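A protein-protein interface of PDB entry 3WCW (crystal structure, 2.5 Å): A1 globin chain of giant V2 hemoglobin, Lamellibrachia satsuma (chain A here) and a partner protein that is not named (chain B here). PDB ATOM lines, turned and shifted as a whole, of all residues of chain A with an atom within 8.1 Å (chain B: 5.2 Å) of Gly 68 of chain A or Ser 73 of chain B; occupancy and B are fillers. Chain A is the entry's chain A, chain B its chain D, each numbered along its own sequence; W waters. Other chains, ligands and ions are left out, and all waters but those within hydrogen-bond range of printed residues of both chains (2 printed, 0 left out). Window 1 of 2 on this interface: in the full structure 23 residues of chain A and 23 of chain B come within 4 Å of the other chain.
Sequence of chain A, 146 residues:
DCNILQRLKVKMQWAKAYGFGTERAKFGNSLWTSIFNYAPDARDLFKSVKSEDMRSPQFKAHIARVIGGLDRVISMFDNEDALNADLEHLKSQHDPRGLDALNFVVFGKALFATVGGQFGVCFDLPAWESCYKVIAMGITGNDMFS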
ATOM      1  N   TRP A  14      30.590  -4.586  25.856  1.00  0.00           N
ATOM      2  CA  TRP A  14      30.180  -5.581  24.873  1.00  0.00           C
ATOM      3  C   TRP A  14      29.378  -4.949  23.729  1.00  0.00           C
ATOM      4  O   TRP A  14      29.620  -5.240  22.551  1.00  0.00           O
ATOM      5  CB  TRP A  14      29.348  -6.683  25.548  1.00  0.00           C
ATOM      6  CG  TRP A  14      28.499  -7.478  24.592  1.00  0.00           C
ATOM      7  CD1 TRP A  14      27.166  -7.297  24.323  1.00  0.00           C
ATOM      8  CD2 TRP A  14      28.944  -8.519  23.718  1.00  0.00           C
ATOM      9  NE1 TRP A  14      26.756  -8.160  23.330  1.00  0.00           N
ATOM     10  CE2 TRP A  14      27.824  -8.923  22.944  1.00  0.00           C
ATOM     11  CE3 TRP A  14      30.178  -9.149  23.510  1.00  0.00           C
ATOM     12  CZ2 TRP A  14      27.904  -9.921  21.991  1.00  0.00           C
ATOM     13  CZ3 TRP A  14      30.256 -10.141  22.565  1.00  0.00           C
ATOM     14  CH2 TRP A  14      29.124 -10.522  21.814  1.00  0.00           C
ATOM     15  N   TYR A  18      30.710  -5.299  19.907  1.00  0.00           N
ATOM     16  CA  TYR A  18      29.883  -6.183  19.085  1.00  0.00           C
ATOM     17  C   TYR A  18      29.321  -5.431  17.874  1.00  0.00           C
ATOM     18  O   TYR A  18      29.217  -5.983  16.780  1.00  0.00           O
ATOM     19  CB  TYR A  18      28.746  -6.724  19.944  1.00  0.00           C
ATOM     20  CG  TYR A  18      27.824  -7.694  19.263  1.00  0.00           C
ATOM     21  CD1 TYR A  18      28.317  -8.849  18.652  1.00  0.00           C
ATOM     22  CD2 TYR A  18      26.445  -7.512  19.318  1.00  0.00           C
ATOM     23  CE1 TYR A  18      27.448  -9.814  18.124  1.00  0.00           C
ATOM     24  CE2 TYR A  18      25.572  -8.462  18.799  1.00  0.00           C
ATOM     25  CZ  TYR A  18      26.078  -9.615  18.210  1.00  0.00           C
ATOM     26  OH  TYR A  18      25.200 -10.576  17.753  1.00  0.00           O
ATOM     27  N   ARG A  24      29.225  -7.304  13.412  1.00  0.00           N
ATOM     28  CA  ARG A  24      29.101  -8.437  14.324  1.00  0.00           C
ATOM     29  C   ARG A  24      29.766  -9.664  13.721  1.00  0.00           C
ATOM     30  O   ARG A  24      30.359 -10.474  14.432  1.00  0.00           O
ATOM     31  CB  ARG A  24      27.637  -8.761  14.600  1.00  0.00           C
ATOM     32  CG  ARG A  24      26.908  -7.711  15.386  1.00  0.00           C
ATOM     33  CD  ARG A  24      25.436  -8.042  15.420  1.00  0.00           C
ATOM     34  NE  ARG A  24      24.634  -6.976  16.005  1.00  0.00           N
ATOM     35  CZ  ARG A  24      23.309  -6.984  16.003  1.00  0.00           C
ATOM     36  NH1 ARG A  24      22.667  -8.009  15.443  1.00  0.00           N
ATOM     37  NH2 ARG A  24      22.630  -5.979  16.550  1.00  0.00           N
ATOM     38  N   ALA A  61      27.350 -19.626  10.182  1.00  0.00           N
ATOM     39  CA  ALA A  61      26.072 -19.766  10.861  1.00  0.00           C
ATOM     40  C   ALA A  61      26.363 -20.097  12.336  1.00  0.00           C
ATOM     41  O   ALA A  61      25.667 -19.647  13.257  1.00  0.00           O
ATOM     42  CB  ALA A  61      25.271 -20.887  10.214  1.00  0.00           C
ATOM     43  N   HIS A  62      27.401 -20.896  12.547  1.00  0.00           N
ATOM     44  CA  HIS A  62      27.793 -21.272  13.892  1.00  0.00           C
ATOM     45  C   HIS A  62      28.333 -20.049  14.620  1.00  0.00           C
ATOM     46  O   HIS A  62      27.984 -19.818  15.783  1.00  0.00           O
ATOM     47  CB  HIS A  62      28.866 -22.357  13.861  1.00  0.00           C
ATOM     48  CG  HIS A  62      29.431 -22.672  15.206  1.00  0.00           C
ATOM     49  ND1 HIS A  62      28.709 -23.332  16.178  1.00  0.00           N
ATOM     50  CD2 HIS A  62      30.629 -22.369  15.762  1.00  0.00           C
ATOM     51  CE1 HIS A  62      29.440 -23.419  17.279  1.00  0.00           C
ATOM     52  NE2 HIS A  62      30.609 -22.842  17.053  1.00  0.00           N
ATOM     53  N   ILE A  63      29.181 -19.278  13.938  1.00  0.00           N
ATOM     54  CA  ILE A  63      29.758 -18.076  14.528  1.00  0.00           C
ATOM     55  C   ILE A  63      28.637 -17.138  14.984  1.00  0.00           C
ATOM     56  O   ILE A  63      28.700 -16.548  16.065  1.00  0.00           O
ATOM     57  CB  ILE A  63      30.640 -17.318  13.522  1.00  0.00           C
ATOM     58  CG1 ILE A  63      31.884 -18.145  13.197  1.00  0.00           C
ATOM     59  CG2 ILE A  63      31.012 -15.943  14.083  1.00  0.00           C
ATOM     60  CD1 ILE A  63      32.816 -17.487  12.188  1.00  0.00           C
ATOM     61  N   ALA A  64      27.607 -17.030  14.154  1.00  0.00           N
ATOM     62  CA  ALA A  64      26.467 -16.173  14.444  1.00  0.00           C
ATOM     63  C   ALA A  64      25.667 -16.648  15.655  1.00  0.00           C
ATOM     64  O   ALA A  64      25.208 -15.824  16.455  1.00  0.00           O
ATOM     65  CB  ALA A  64      25.546 -16.081  13.211  1.00  0.00           C
ATOM     66  N   ARG A  65      25.493 -17.962  15.792  1.00  0.00           N
ATOM     67  CA  ARG A  65      24.723 -18.491  16.917  1.00  0.00           C
ATOM     68  C   ARG A  65      25.471 -18.314  18.231  1.00  0.00           C
ATOM     69  O   ARG A  65      24.880 -17.987  19.253  1.00  0.00           O
ATOM     70  CB  ARG A  65      24.367 -19.976  16.691  1.00  0.00           C
ATOM     71  CG  ARG A  65      23.202 -20.202  15.699  1.00  0.00           C
ATOM     72  CD  ARG A  65      22.710 -21.664  15.658  1.00  0.00           C
ATOM     73  NE  ARG A  65      23.734 -22.596  15.187  1.00  0.00           N
ATOM     74  CZ  ARG A  65      23.985 -22.876  13.910  1.00  0.00           C
ATOM     75  NH1 ARG A  65      23.282 -22.306  12.936  1.00  0.00           N
ATOM     76  NH2 ARG A  65      24.963 -23.715  13.602  1.00  0.00           N
ATOM     77  N   VAL A  66      26.785 -18.497  18.183  1.00  0.00           N
ATOM     78  CA  VAL A  66      27.614 -18.359  19.365  1.00  0.00           C
ATOM     79  C   VAL A  66      27.682 -16.934  19.884  1.00  0.00           C
ATOM     80  O   VAL A  66      27.584 -16.712  21.089  1.00  0.00           O
ATOM     81  CB  VAL A  66      29.049 -18.835  19.101  1.00  0.00           C
ATOM     82  CG1 VAL A  66      29.884 -18.662  20.358  1.00  0.00           C
ATOM     83  CG2 VAL A  66      29.045 -20.301  18.651  1.00  0.00           C
ATOM     84  N   ILE A  67      27.861 -15.961  18.996  1.00  0.00           N
ATOM     85  CA  ILE A  67      27.934 -14.578  19.461  1.00  0.00           C
ATOM     86  C   ILE A  67      26.544 -14.041  19.809  1.00  0.00           C
ATOM     87  O   ILE A  67      26.407 -13.126  20.628  1.00  0.00           O
ATOM     88  CB  ILE A  67      28.624 -13.669  18.426  1.00  0.00           C
ATOM     89  CG1 ILE A  67      27.791 -13.596  17.149  1.00  0.00           C
ATOM     90  CG2 ILE A  67      30.032 -14.195  18.149  1.00  0.00           C
ATOM     91  CD1 ILE A  67      28.408 -12.739  16.081  1.00  0.00           C
ATOM     92  N   GLY A  68      25.516 -14.610  19.183  1.00  0.00           N
ATOM     93  CA  GLY A  68      24.155 -14.208  19.493  1.00  0.00           C
ATOM     94  C   GLY A  68      23.857 -14.697  20.906  1.00  0.00           C
ATOM     95  O   GLY A  68      23.097 -14.058  21.651  1.00  0.00           O
ATOM     96  N   GLY A  69      24.475 -15.828  21.274  1.00  0.00           N
ATOM     97  CA  GLY A  69      24.310 -16.411  22.599  1.00  0.00           C
ATOM     98  C   GLY A  69      25.039 -15.578  23.648  1.00  0.00           C
ATOM     99  O   GLY A  69      24.575 -15.412  24.777  1.00  0.00           O
ATOM    100  N   LEU A  70      26.194 -15.046  23.276  1.00  0.00           N
ATOM    101  CA  LEU A  70      26.956 -14.205  24.194  1.00  0.00           C
ATOM    102  C   LEU A  70      26.138 -12.955  24.483  1.00  0.00           C
ATOM    103  O   LEU A  70      26.083 -12.476  25.618  1.00  0.00           O
ATOM    104  CB  LEU A  70      28.293 -13.795  23.570  1.00  0.00           C
ATOM    105  CG  LEU A  70      29.389 -14.843  23.674  1.00  0.00           C
ATOM    106  CD1 LEU A  70      30.638 -14.395  22.919  1.00  0.00           C
ATOM    107  CD2 LEU A  70      29.684 -15.059  25.154  1.00  0.00           C
ATOM    108  N   ASP A  71      25.501 -12.441  23.438  1.00  0.00           N
ATOM    109  CA  ASP A  71      24.700 -11.244  23.534  1.00  0.00           C
ATOM    110  C   ASP A  71      23.472 -11.424  24.401  1.00  0.00           C
ATOM    111  O   ASP A  71      23.229 -10.627  25.301  1.00  0.00           O
ATOM    112  CB  ASP A  71      24.268 -10.787  22.141  1.00  0.00           C
ATOM    113  CG  ASP A  71      23.388  -9.562  22.192  1.00  0.00           C
ATOM    114  OD1 ASP A  71      23.937  -8.472  22.413  1.00  0.00           O
ATOM    115  OD2 ASP A  71      22.150  -9.696  22.038  1.00  0.00           O
ATOM    116  N   ARG A  72      22.683 -12.461  24.132  1.00  0.00           N
ATOM    117  CA  ARG A  72      21.475 -12.680  24.932  1.00  0.00           C
ATOM    118  C   ARG A  72      21.810 -12.979  26.395  1.00  0.00           C
ATOM    119  O   ARG A  72      21.113 -12.527  27.298  1.00  0.00           O
ATOM    120  CB  ARG A  72      20.618 -13.806  24.338  1.00  0.00           C
ATOM    121  CG  ARG A  72      21.147 -15.215  24.492  1.00  0.00           C
ATOM    122  CD  ARG A  72      20.207 -16.163  23.761  1.00  0.00           C
ATOM    123  NE  ARG A  72      20.111 -17.440  24.448  1.00  0.00           N
ATOM    124  CZ  ARG A  72      20.544 -18.595  23.957  1.00  0.00           C
ATOM    125  NH1 ARG A  72      21.105 -18.645  22.761  1.00  0.00           N
ATOM    126  NH2 ARG A  72      20.427 -19.701  24.680  1.00  0.00           N
ATOM    127  N   VAL A  73      22.886 -13.725  26.619  1.00  0.00           N
ATOM    128  CA  VAL A  73      23.308 -14.044  27.969  1.00  0.00           C
ATOM    129  C   VAL A  73      23.769 -12.755  28.654  1.00  0.00           C
ATOM    130  O   VAL A  73      23.333 -12.450  29.761  1.00  0.00           O
ATOM    131  CB  VAL A  73      24.441 -15.112  27.950  1.00  0.00           C
ATOM    132  CG1 VAL A  73      25.253 -15.050  29.210  1.00  0.00           C
ATOM    133  CG2 VAL A  73      23.834 -16.492  27.786  1.00  0.00           C
ATOM    134  N   ILE A  74      24.627 -11.978  27.998  1.00  0.00           N
ATOM    135  CA  ILE A  74      25.080 -10.726  28.602  1.00  0.00           C
ATOM    136  C   ILE A  74      23.909  -9.772  28.854  1.00  0.00           C
ATOM    137  O   ILE A  74      23.891  -9.056  29.865  1.00  0.00           O
ATOM    138  CB  ILE A  74      26.165 -10.024  27.727  1.00  0.00           C
ATOM    139  CG1 ILE A  74      27.502 -10.766  27.897  1.00  0.00           C
ATOM    140  CG2 ILE A  74      26.288  -8.544  28.106  1.00  0.00           C
ATOM    141  CD1 ILE A  74      28.586 -10.408  26.870  1.00  0.00           C
ATOM    142  N   SER A  75      22.921  -9.771  27.962  1.00  0.00           N
ATOM    143  CA  SER A  75      21.779  -8.885  28.148  1.00  0.00           C
ATOM    144  C   SER A  75      20.944  -9.288  29.362  1.00  0.00           C
ATOM    145  O   SER A  75      20.224  -8.472  29.917  1.00  0.00           O
ATOM    146  CB  SER A  75      20.904  -8.846  26.891  1.00  0.00           C
ATOM    147  OG  SER A  75      19.783  -9.697  27.010  1.00  0.00           O
ATOM    148  N   MET A  76      21.054 -10.542  29.786  1.00  0.00           N
ATOM    149  CA  MET A  76      20.314 -11.009  30.957  1.00  0.00           C
ATOM    150  C   MET A  76      21.119 -10.897  32.263  1.00  0.00           C
ATOM    151  O   MET A  76      20.601 -11.153  33.345  1.00  0.00           O
ATOM    152  CB  MET A  76      19.851 -12.454  30.744  1.00  0.00           C
ATOM    153  CG  MET A  76      18.710 -12.574  29.742  1.00  0.00           C
ATOM    154  SD  MET A  76      18.087 -14.259  29.563  1.00  0.00           S
ATOM    155  CE  MET A  76      19.243 -14.897  28.363  1.00  0.00           C
ATOM    156  N   ASP A  86      18.671 -19.722  31.086  1.00  0.00           N
ATOM    157  CA  ASP A  86      19.243 -19.796  29.753  1.00  0.00           C
ATOM    158  C   ASP A  86      20.623 -20.431  29.730  1.00  0.00           C
ATOM    159  O   ASP A  86      21.002 -21.049  28.732  1.00  0.00           O
ATOM    160  CB  ASP A  86      19.295 -18.414  29.098  1.00  0.00           C
ATOM    161  CG  ASP A  86      19.546 -18.500  27.605  1.00  0.00           C
ATOM    162  OD1 ASP A  86      18.826 -19.266  26.938  1.00  0.00           O
ATOM    163  OD2 ASP A  86      20.453 -17.817  27.096  1.00  0.00           O
ATOM    164  N   LEU A  90      21.914 -23.697  27.634  1.00  0.00           N
ATOM    165  CA  LEU A  90      23.154 -23.831  26.884  1.00  0.00           C
ATOM    166  C   LEU A  90      23.933 -25.027  27.410  1.00  0.00           C
ATOM    167  O   LEU A  90      24.587 -25.735  26.641  1.00  0.00           O
ATOM    168  CB  LEU A  90      24.016 -22.567  27.011  1.00  0.00           C
ATOM    169  CG  LEU A  90      23.402 -21.229  26.579  1.00  0.00           C
ATOM    170  CD1 LEU A  90      24.376 -20.070  26.803  1.00  0.00           C
ATOM    171  CD2 LEU A  90      23.022 -21.341  25.119  1.00  0.00           C
ATOM    172  N   TYR B  20      15.804  -3.141  19.024  1.00  0.00           N
ATOM    173  CA  TYR B  20      16.560  -4.281  19.525  1.00  0.00           C
ATOM    174  C   TYR B  20      18.041  -4.163  19.205  1.00  0.00           C
ATOM    175  O   TYR B  20      18.425  -3.968  18.055  1.00  0.00           O
ATOM    176  CB  TYR B  20      16.018  -5.584  18.940  1.00  0.00           C
ATOM    177  CG  TYR B  20      16.652  -6.825  19.512  1.00  0.00           C
ATOM    178  CD1 TYR B  20      17.978  -7.157  19.220  1.00  0.00           C
ATOM    179  CD2 TYR B  20      15.929  -7.680  20.338  1.00  0.00           C
ATOM    180  CE1 TYR B  20      18.570  -8.323  19.736  1.00  0.00           C
ATOM    181  CE2 TYR B  20      16.510  -8.846  20.858  1.00  0.00           C
ATOM    182  CZ  TYR B  20      17.830  -9.162  20.548  1.00  0.00           C
ATOM    183  OH  TYR B  20      18.385 -10.339  21.011  1.00  0.00           O
ATOM    184  N   THR B  68      11.732 -16.481  25.311  1.00  0.00           N
ATOM    185  CA  THR B  68      11.473 -15.346  24.431  1.00  0.00           C
ATOM    186  C   THR B  68      12.763 -14.587  24.099  1.00  0.00           C
ATOM    187  O   THR B  68      12.957 -14.144  22.966  1.00  0.00           O
ATOM    188  CB  THR B  68      10.450 -14.373  25.058  1.00  0.00           C
ATOM    189  OG1 THR B  68      11.045 -13.698  26.170  1.00  0.00           O
ATOM    190  CG2 THR B  68       9.227 -15.139  25.550  1.00  0.00           C
ATOM    191  N   VAL B  69      13.643 -14.419  25.082  1.00  0.00           N
ATOM    192  CA  VAL B  69      14.909 -13.734  24.830  1.00  0.00           C
ATOM    193  C   VAL B  69      15.630 -14.513  23.728  1.00  0.00           C
ATOM    194  O   VAL B  69      16.212 -13.934  22.804  1.00  0.00           O
ATOM    195  CB  VAL B  69      15.804 -13.705  26.096  1.00  0.00           C
ATOM    196  CG1 VAL B  69      17.259 -13.495  25.705  1.00  0.00           C
ATOM    197  CG2 VAL B  69      15.363 -12.596  27.018  1.00  0.00           C
ATOM    198  N   ARG B  70      15.559 -15.832  23.831  1.00  0.00           N
ATOM    199  CA  ARG B  70      16.189 -16.738  22.885  1.00  0.00           C
ATOM    200  C   ARG B  70      15.566 -16.638  21.481  1.00  0.00           C
ATOM    201  O   ARG B  70      16.270 -16.733  20.471  1.00  0.00           O
ATOM    202  CB  ARG B  70      16.048 -18.154  23.432  1.00  0.00           C
ATOM    203  CG  ARG B  70      17.144 -19.125  23.085  1.00  0.00           C
ATOM    204  CD  ARG B  70      16.935 -20.438  23.863  1.00  0.00           C
ATOM    205  NE  ARG B  70      17.109 -20.241  25.297  1.00  0.00           N
ATOM    206  CZ  ARG B  70      16.312 -20.750  26.233  1.00  0.00           C
ATOM    207  NH1 ARG B  70      15.266 -21.495  25.892  1.00  0.00           N
ATOM    208  NH2 ARG B  70      16.563 -20.505  27.516  1.00  0.00           N
ATOM    209  N   VAL B  71      14.255 -16.440  21.421  1.00  0.00           N
ATOM    210  CA  VAL B  71      13.541 -16.339  20.145  1.00  0.00           C
ATOM    211  C   VAL B  71      13.821 -15.004  19.449  1.00  0.00           C
ATOM    212  O   VAL B  71      14.102 -14.948  18.236  1.00  0.00           O
ATOM    213  CB  VAL B  71      12.004 -16.494  20.359  1.00  0.00           C
ATOM    214  CG1 VAL B  71      11.249 -16.206  19.060  1.00  0.00           C
ATOM    215  CG2 VAL B  71      11.692 -17.913  20.863  1.00  0.00           C
ATOM    216  N   LEU B  72      13.740 -13.928  20.221  1.00  0.00           N
ATOM    217  CA  LEU B  72      14.008 -12.615  19.681  1.00  0.00           C
ATOM    218  C   LEU B  72      15.465 -12.604  19.204  1.00  0.00           C
ATOM    219  O   LEU B  72      15.789 -11.929  18.232  1.00  0.00           O
ATOM    220  CB  LEU B  72      13.778 -11.549  20.752  1.00  0.00           C
ATOM    221  CG  LEU B  72      12.349 -11.451  21.279  1.00  0.00           C
ATOM    222  CD1 LEU B  72      12.313 -10.398  22.362  1.00  0.00           C
ATOM    223  CD2 LEU B  72      11.375 -11.095  20.157  1.00  0.00           C
ATOM    224  N   SER B  73      16.330 -13.360  19.886  1.00  0.00           N
ATOM    225  CA  SER B  73      17.744 -13.441  19.515  1.00  0.00           C
ATOM    226  C   SER B  73      17.920 -14.146  18.167  1.00  0.00           C
ATOM    227  O   SER B  73      18.812 -13.807  17.385  1.00  0.00           O
ATOM    228  CB  SER B  73      18.539 -14.182  20.594  1.00  0.00           C
ATOM    229  OG  SER B  73      19.888 -14.399  20.186  1.00  0.00           O
ATOM    230  N   GLY B  74      17.074 -15.140  17.902  1.00  0.00           N
ATOM    231  CA  GLY B  74      17.144 -15.838  16.631  1.00  0.00           C
ATOM    232  C   GLY B  74      16.659 -14.912  15.522  1.00  0.00           C
ATOM    233  O   GLY B  74      17.272 -14.802  14.454  1.00  0.00           O
ATOM    234  N   LEU B  75      15.544 -14.241  15.784  1.00  0.00           N
ATOM    235  CA  LEU B  75      14.967 -13.306  14.825  1.00  0.00           C
ATOM    236  C   LEU B  75      16.048 -12.266  14.501  1.00  0.00           C
ATOM    237  O   LEU B  75      16.234 -11.887  13.348  1.00  0.00           O
ATOM    238  CB  LEU B  75      13.742 -12.632  15.446  1.00  0.00           C
ATOM    239  CG  LEU B  75      12.861 -11.761  14.569  1.00  0.00           C
ATOM    240  CD1 LEU B  75      12.264 -12.588  13.447  1.00  0.00           C
ATOM    241  CD2 LEU B  75      11.753 -11.174  15.421  1.00  0.00           C
ATOM    242  N   ASP B  76      16.761 -11.826  15.536  1.00  0.00           N
ATOM    243  CA  ASP B  76      17.827 -10.850  15.386  1.00  0.00           C
ATOM    244  C   ASP B  76      18.887 -11.369  14.437  1.00  0.00           C
ATOM    245  O   ASP B  76      19.368 -10.626  13.577  1.00  0.00           O
ATOM    246  CB  ASP B  76      18.462 -10.542  16.738  1.00  0.00           C
ATOM    247  CG  ASP B  76      19.559  -9.497  16.640  1.00  0.00           C
ATOM    248  OD1 ASP B  76      20.754  -9.846  16.850  1.00  0.00           O
ATOM    249  OD2 ASP B  76      19.223  -8.327  16.349  1.00  0.00           O
ATOM    250  N   MET B  77      19.252 -12.639  14.587  1.00  0.00           N
ATOM    251  CA  MET B  77      20.258 -13.226  13.713  1.00  0.00           C
ATOM    252  C   MET B  77      19.779 -13.283  12.282  1.00  0.00           C
ATOM    253  O   MET B  77      20.546 -13.026  11.366  1.00  0.00           O
ATOM    254  CB  MET B  77      20.599 -14.638  14.139  1.00  0.00           C
ATOM    255  CG  MET B  77      21.529 -14.731  15.302  1.00  0.00           C
ATOM    256  SD  MET B  77      21.624 -16.460  15.755  1.00  0.00           S
ATOM    257  CE  MET B  77      22.449 -17.076  14.342  1.00  0.00           C
HETATM  258  O   HOH W   1      23.438 -10.583  15.123  1.00  0.00           O
HETATM  259  O   HOH W   2      20.832 -16.860  20.328  1.00  0.00           O
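N of Arg 65 of chain A touches CE of Met 77 of chain B, 3.5 Å away.
O of Gly 68 of chain A touches OG of Ser 73 of chain B, at 3.5 Å.
Asp 71 of chain A touches Tyr 20 of chain B.
Arg 72 of chain A touches Val 69 of chain B.
Ser 73 of chain B touches Arg 72 of chain A.
Met 76 of chain A touches Val 69 of chain B (CE to CG1, 3.6 Å).
Of the 11 printed residues of chain B, 6 touch a printed residue of chain A.
Hydrophobic or aromatic side chains of chain B that line the printed part of chain A: Tyr 20, Val 69 and Met 77.
Printed residues of chain A that touch a printed residue of chain B: Arg 24, Ala 64, Arg 65, Gly 68, Asp 71, Arg 72, Met 76 and Asp 86.
Hydrophobic or aromatic side chains of chain A that line the printed part of chain B: Ala 64 and Met 76.
Among the printed residues, 10 pairs touch across the chains.
The backbone carbonyl oxygen (O) of Arg 72 of chain A lies within hydrogen-bond range of the side-chain hydroxyl (OG) of Ser 75 of chain A (3.1 Å).
The indole nitrogen (NE1) of Trp 14 of chain A lies within hydrogen-bond range of the side-chain carboxylate (OD1) of Asp 71 of chain A.
The guanidinium group (NE) of Arg 72 of chain A lies within salt-bridge range of the side-chain carboxylate (OD2) of Asp 86 of chain A, at 2.7 Å.
Of the printed residues of chain B, Arg 24 of chain A touches Asp 76.
Of the printed residues of chain B, Ala 64 of chain A touches Met 77.
Gly 68 of chain A touches one residue of chain B.
Of the printed residues of chain A, Val 69 of chain B touches Arg 72 and Met 76.
Printed residues of chain A within 4 Å of Arg 70 of chain B: Arg 72 and Asp 86.
Of the printed residues of chain A, Ser 73 of chain B touches Gly 68 (3.5 Å) and Arg 72 (3.999 Å).
No residue of chain A comes within 4 Å of Gly 74 of chain B.
Of the printed residues of chain A, Met 77 of chain B touches Ala 64 (3.4 Å) and Arg 65 (3.5 Å).
The nearest residue of chain B that does not touch Gly 68 of chain A is Met 77 of chain B (5.0 Å).
The nearest printed residue of chain A that does not touch Ser 73 of chain B is Gly 69 of chain A (4.9 Å).
Water W2 lies within hydrogen-bond range of OG of Ser 73 of chain B (2.6 Å) and NH1 of Arg 72 of chain A (3.0 Å).
Water W1 lies within hydrogen-bond range of the guanidinium group of Arg 24 of chain A (2.7 Å), the side-chain hydroxyl of Tyr 18 of chain A (3.2 Å) and the side-chain carboxylate of Asp 76 of chain B (3.3 Å).
The side-chain carboxylate of Asp 86 of chain A is in salt-bridge range of the guanidinium group of Arg 70 of chain B (2.6 Å).
The guanidinium group (NH1) of Arg 24 of chain A is in salt-bridge range of the side-chain carboxylate (OD1) of Asp 76 of chain B (3.0 Å).
The guanidinium group (NH2) of Arg 72 of chain A lies close to the guanidinium group (NE) of Arg 70 of chain B (3.4 Å).
The backbone carbonyl oxygen (O) of Ala 64 of chain A lies close to the side-chain sulfur (SD) of Met 77 of chain B (3.7 Å).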
